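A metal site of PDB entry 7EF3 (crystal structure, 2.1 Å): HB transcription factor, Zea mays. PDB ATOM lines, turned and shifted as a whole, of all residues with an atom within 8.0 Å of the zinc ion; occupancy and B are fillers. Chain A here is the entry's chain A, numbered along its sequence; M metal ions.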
ATOM      1  N   GLU A  70     -30.385  10.565  20.212  1.00  0.00           N
ATOM      2  CA  GLU A  70     -31.685  11.099  19.873  1.00  0.00           C
ATOM      3  C   GLU A  70     -31.453  12.326  19.005  1.00  0.00           C
ATOM      4  O   GLU A  70     -30.424  12.988  19.129  1.00  0.00           O
ATOM      5  CB  GLU A  70     -32.487  11.466  21.130  1.00  0.00           C
ATOM      6  CG  GLU A  70     -32.706  10.319  22.090  1.00  0.00           C
ATOM      7  CD  GLU A  70     -34.025   9.621  21.874  1.00  0.00           C
ATOM      8  OE1 GLU A  70     -35.061  10.103  22.379  1.00  0.00           O
ATOM      9  OE2 GLU A  70     -34.042   8.576  21.195  1.00  0.00           O
ATOM     10  N   ALA A  71     -32.401  12.630  18.115  1.00  0.00           N
ATOM     11  CA  ALA A  71     -32.279  13.778  17.215  1.00  0.00           C
ATOM     12  C   ALA A  71     -32.081  15.071  18.004  1.00  0.00           C
ATOM     13  O   ALA A  71     -31.389  15.991  17.551  1.00  0.00           O
ATOM     14  CB  ALA A  71     -33.493  13.888  16.316  1.00  0.00           C
ATOM     15  N   THR A  72     -32.683  15.137  19.186  1.00  0.00           N
ATOM     16  CA  THR A  72     -32.586  16.286  20.078  1.00  0.00           C
ATOM     17  C   THR A  72     -31.171  16.453  20.628  1.00  0.00           C
ATOM     18  O   THR A  72     -30.681  17.585  20.798  1.00  0.00           O
ATOM     19  CB  THR A  72     -33.590  16.154  21.247  1.00  0.00           C
ATOM     20  OG1 THR A  72     -34.906  16.496  20.796  1.00  0.00           O
ATOM     21  CG2 THR A  72     -33.208  17.073  22.408  1.00  0.00           C
ATOM     22  N   GLU A  73     -30.499  15.338  20.874  1.00  0.00           N
ATOM     23  CA  GLU A  73     -29.232  15.330  21.592  1.00  0.00           C
ATOM     24  C   GLU A  73     -28.027  15.786  20.763  1.00  0.00           C
ATOM     25  O   GLU A  73     -26.888  15.676  21.224  1.00  0.00           O
ATOM     26  CB  GLU A  73     -28.972  13.938  22.151  1.00  0.00           C
ATOM     27  CG  GLU A  73     -30.062  13.430  23.071  1.00  0.00           C
ATOM     28  CD  GLU A  73     -29.897  11.958  23.405  1.00  0.00           C
ATOM     29  OE1 GLU A  73     -29.103  11.274  22.725  1.00  0.00           O
ATOM     30  OE2 GLU A  73     -30.560  11.488  24.342  1.00  0.00           O
ATOM     31  N   CYS A  74     -28.274  16.291  19.553  1.00  0.00           N
ATOM     32  CA  CYS A  74     -27.186  16.766  18.696  1.00  0.00           C
ATOM     33  C   CYS A  74     -26.422  17.913  19.356  1.00  0.00           C
ATOM     34  O   CYS A  74     -25.259  18.162  19.035  1.00  0.00           O
ATOM     35  CB  CYS A  74     -27.726  17.201  17.333  1.00  0.00           C
ATOM     36  SG  CYS A  74     -28.937  18.528  17.418  1.00  0.00           S
ATOM     37  N   VAL A  75     -27.076  18.613  20.282  1.00  0.00           N
ATOM     38  CA  VAL A  75     -26.467  19.736  20.995  1.00  0.00           C
ATOM     39  C   VAL A  75     -25.444  19.265  22.016  1.00  0.00           C
ATOM     40  O   VAL A  75     -24.727  20.064  22.613  1.00  0.00           O
ATOM     41  CB  VAL A  75     -27.544  20.597  21.696  1.00  0.00           C
ATOM     42  CG1 VAL A  75     -28.440  21.258  20.659  1.00  0.00           C
ATOM     43  CG2 VAL A  75     -28.359  19.732  22.646  1.00  0.00           C
ATOM     44  N   GLN A 104     -21.697  21.574  11.506  1.00  0.00           N
ATOM     45  CA  GLN A 104     -22.612  22.486  10.835  1.00  0.00           C
ATOM     46  C   GLN A 104     -24.034  22.204  11.309  1.00  0.00           C
ATOM     47  O   GLN A 104     -24.638  21.202  10.928  1.00  0.00           O
ATOM     48  CB  GLN A 104     -22.524  22.356   9.313  1.00  0.00           C
ATOM     49  CG  GLN A 104     -23.282  23.458   8.568  1.00  0.00           C
ATOM     50  CD  GLN A 104     -23.548  23.124   7.114  1.00  0.00           C
ATOM     51  OE1 GLN A 104     -23.737  21.955   6.758  1.00  0.00           O
ATOM     52  NE2 GLN A 104     -23.568  24.142   6.267  1.00  0.00           N
ATOM     53  N   ARG A 105     -24.564  23.081  12.147  1.00  0.00           N
ATOM     54  CA  ARG A 105     -25.868  22.869  12.749  1.00  0.00           C
ATOM     55  C   ARG A 105     -26.965  23.544  11.940  1.00  0.00           C
ATOM     56  O   ARG A 105     -26.941  24.761  11.734  1.00  0.00           O
ATOM     57  CB  ARG A 105     -25.878  23.345  14.197  1.00  0.00           C
ATOM     58  CG  ARG A 105     -24.673  22.818  14.979  1.00  0.00           C
ATOM     59  CD  ARG A 105     -24.774  23.089  16.471  1.00  0.00           C
ATOM     60  NE  ARG A 105     -23.543  22.732  17.162  1.00  0.00           N
ATOM     61  CZ  ARG A 105     -23.271  21.523  17.645  1.00  0.00           C
ATOM     62  NH1 ARG A 105     -24.160  20.536  17.519  1.00  0.00           N
ATOM     63  NH2 ARG A 105     -22.118  21.291  18.250  1.00  0.00           N
ATOM     64  N   ARG A 106     -27.919  22.752  11.475  1.00  0.00           N
ATOM     65  CA  ARG A 106     -29.002  23.245  10.638  1.00  0.00           C
ATOM     66  C   ARG A 106     -30.355  22.933  11.273  1.00  0.00           C
ATOM     67  O   ARG A 106     -30.444  22.072  12.131  1.00  0.00           O
ATOM     68  CB  ARG A 106     -28.920  22.632   9.237  1.00  0.00           C
ATOM     69  CG  ARG A 106     -27.518  22.657   8.651  1.00  0.00           C
ATOM     70  CD  ARG A 106     -27.486  22.161   7.213  1.00  0.00           C
ATOM     71  NE  ARG A 106     -27.793  20.734   7.124  1.00  0.00           N
ATOM     72  CZ  ARG A 106     -27.697  20.029   5.998  1.00  0.00           C
ATOM     73  NH1 ARG A 106     -27.312  20.617   4.887  1.00  0.00           N
ATOM     74  NH2 ARG A 106     -27.990  18.731   6.000  1.00  0.00           N
ATOM     75  N   ARG A 107     -31.400  23.663  10.863  1.00  0.00           N
ATOM     76  CA  ARG A 107     -32.709  23.479  11.450  1.00  0.00           C
ATOM     77  C   ARG A 107     -33.220  22.065  11.171  1.00  0.00           C
ATOM     78  O   ARG A 107     -33.072  21.542  10.071  1.00  0.00           O
ATOM     79  CB  ARG A 107     -33.705  24.530  10.947  1.00  0.00           C
ATOM     80  CG  ARG A 107     -34.067  24.432   9.473  1.00  0.00           C
ATOM     81  CD  ARG A 107     -35.301  25.236   9.146  1.00  0.00           C
ATOM     82  NE  ARG A 107     -35.887  24.843   7.863  1.00  0.00           N
ATOM     83  CZ  ARG A 107     -36.751  23.838   7.722  1.00  0.00           C
ATOM     84  NH1 ARG A 107     -37.135  23.132   8.772  1.00  0.00           N
ATOM     85  NH2 ARG A 107     -37.235  23.544   6.517  1.00  0.00           N
ATOM     86  N   HIS A 108     -33.825  21.452  12.182  1.00  0.00           N
ATOM     87  CA  HIS A 108     -34.356  20.107  12.060  1.00  0.00           C
ATOM     88  C   HIS A 108     -35.607  20.083  11.187  1.00  0.00           C
ATOM     89  O   HIS A 108     -36.192  21.120  10.889  1.00  0.00           O
ATOM     90  CB  HIS A 108     -34.682  19.520  13.429  1.00  0.00           C
ATOM     91  CG  HIS A 108     -33.477  19.201  14.248  1.00  0.00           C
ATOM     92  ND1 HIS A 108     -33.563  18.566  15.474  1.00  0.00           N
ATOM     93  CD2 HIS A 108     -32.158  19.415  14.030  1.00  0.00           C
ATOM     94  CE1 HIS A 108     -32.347  18.404  15.970  1.00  0.00           C
ATOM     95  NE2 HIS A 108     -31.474  18.910  15.118  1.00  0.00           N
ATOM     96  N   GLY A 112     -35.919  14.558  11.432  1.00  0.00           N
ATOM     97  CA  GLY A 112     -35.089  14.664  12.619  1.00  0.00           C
ATOM     98  C   GLY A 112     -33.912  15.603  12.452  1.00  0.00           C
ATOM     99  O   GLY A 112     -34.041  16.692  11.890  1.00  0.00           O
ATOM    100  N   CYS A 113     -32.753  15.171  12.925  1.00  0.00           N
ATOM    101  CA  CYS A 113     -31.558  16.005  12.904  1.00  0.00           C
ATOM    102  C   CYS A 113     -30.984  16.144  11.489  1.00  0.00           C
ATOM    103  O   CYS A 113     -30.831  15.152  10.774  1.00  0.00           O
ATOM    104  CB  CYS A 113     -30.495  15.437  13.838  1.00  0.00           C
ATOM    105  SG  CYS A 113     -28.948  16.360  13.845  1.00  0.00           S
ATOM    106  N   ARG A 114     -30.666  17.375  11.103  1.00  0.00           N
ATOM    107  CA  ARG A 114     -30.086  17.648   9.798  1.00  0.00           C
ATOM    108  C   ARG A 114     -28.664  18.189   9.935  1.00  0.00           C
ATOM    109  O   ARG A 114     -28.082  18.674   8.970  1.00  0.00           O
ATOM    110  CB  ARG A 114     -30.954  18.647   9.022  1.00  0.00           C
ATOM    111  CG  ARG A 114     -32.257  18.055   8.500  1.00  0.00           C
ATOM    112  CD  ARG A 114     -33.162  19.119   7.896  1.00  0.00           C
ATOM    113  NE  ARG A 114     -32.544  19.809   6.775  1.00  0.00           N
ATOM    114  CZ  ARG A 114     -32.048  21.040   6.834  1.00  0.00           C
ATOM    115  NH1 ARG A 114     -32.094  21.716   7.973  1.00  0.00           N
ATOM    116  NH2 ARG A 114     -31.505  21.596   5.755  1.00  0.00           N
ATOM    117  N   CYS A 115     -28.114  18.094  11.139  1.00  0.00           N
ATOM    118  CA  CYS A 115     -26.769  18.598  11.389  1.00  0.00           C
ATOM    119  C   CYS A 115     -25.706  17.684  10.796  1.00  0.00           C
ATOM    120  O   CYS A 115     -25.869  16.460  10.774  1.00  0.00           O
ATOM    121  CB  CYS A 115     -26.543  18.773  12.896  1.00  0.00           C
ATOM    122  SG  CYS A 115     -27.725  19.866  13.704  1.00  0.00           S
ATOM    123  N   ARG A 116     -24.625  18.278  10.307  1.00  0.00           N
ATOM    124  CA  ARG A 116     -23.481  17.517   9.799  1.00  0.00           C
ATOM    125  C   ARG A 116     -22.302  17.657  10.760  1.00  0.00           C
ATOM    126  O   ARG A 116     -22.105  18.718  11.343  1.00  0.00           O
ATOM    127  CB  ARG A 116     -23.086  18.002   8.401  1.00  0.00           C
ATOM    128  CG  ARG A 116     -24.239  18.410   7.499  1.00  0.00           C
ATOM    129  CD  ARG A 116     -25.174  17.256   7.191  1.00  0.00           C
ATOM    130  NE  ARG A 116     -24.451  16.044   6.817  1.00  0.00           N
ATOM    131  CZ  ARG A 116     -25.022  14.980   6.253  1.00  0.00           C
ATOM    132  NH1 ARG A 116     -24.281  13.925   5.942  1.00  0.00           N
ATOM    133  NH2 ARG A 116     -26.322  14.982   5.981  1.00  0.00           N
ATOM    134  N   PHE A 117     -21.521  16.592  10.906  1.00  0.00           N
ATOM    135  CA  PHE A 117     -20.346  16.637  11.782  1.00  0.00           C
ATOM    136  C   PHE A 117     -19.095  16.205  11.037  1.00  0.00           C
ATOM    137  O   PHE A 117     -19.026  15.104  10.498  1.00  0.00           O
ATOM    138  CB  PHE A 117     -20.555  15.745  13.014  1.00  0.00           C
ATOM    139  CG  PHE A 117     -21.707  16.159  13.888  1.00  0.00           C
ATOM    140  CD1 PHE A 117     -22.970  15.625  13.684  1.00  0.00           C
ATOM    141  CD2 PHE A 117     -21.537  17.082  14.897  1.00  0.00           C
ATOM    142  CE1 PHE A 117     -24.036  16.001  14.484  1.00  0.00           C
ATOM    143  CE2 PHE A 117     -22.593  17.467  15.703  1.00  0.00           C
ATOM    144  CZ  PHE A 117     -23.843  16.924  15.493  1.00  0.00           C
ATOM    145  N   LEU A 132     -25.964  12.625  12.298  1.00  0.00           N
ATOM    146  CA  LEU A 132     -26.094  12.256  13.701  1.00  0.00           C
ATOM    147  C   LEU A 132     -26.379  10.760  13.875  1.00  0.00           C
ATOM    148  O   LEU A 132     -26.002  10.167  14.888  1.00  0.00           O
ATOM    149  CB  LEU A 132     -27.195  13.078  14.379  1.00  0.00           C
ATOM    150  CG  LEU A 132     -27.331  12.925  15.895  1.00  0.00           C
ATOM    151  CD1 LEU A 132     -26.102  13.494  16.602  1.00  0.00           C
ATOM    152  CD2 LEU A 132     -28.593  13.594  16.400  1.00  0.00           C
HETATM  153 ZN    ZN M   1     -29.187  18.464  15.015  1.00  0.00          ZN
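Of the 18 residues printed, 4 come within 4 Å of the zinc ion.
Along chain A the residues within 4 Å of the zinc ion span positions 74 to 115.
The nearest printed residue that does not touch the zinc ion is Ala 71 (4.2 Å).
O of Cys 74 is in hydrogen-bond range of NH1 of Arg 105.
The side-chain sulfur (SG) of Cys 115 sits close to the backbone NH (N) of Arg 106 (3.7 Å).
The backbone carbonyl oxygen of Ala 71 sits close to the side-chain sulfur of Cys 74, at 3.5 Å.
The zinc ion is bound by a ring nitrogen (NE2) of His 108 (2.3 Å).
SG of Cys 115 is bound to the zinc ion (2.4 Å).
SG of Cys 74 is bound to the zinc ion, at 2.4 Å.
The zinc ion is bound by the side-chain sulfur (SG) of Cys 113, 2.4 Å away.
The zinc ion has four donor atoms within binding distance.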
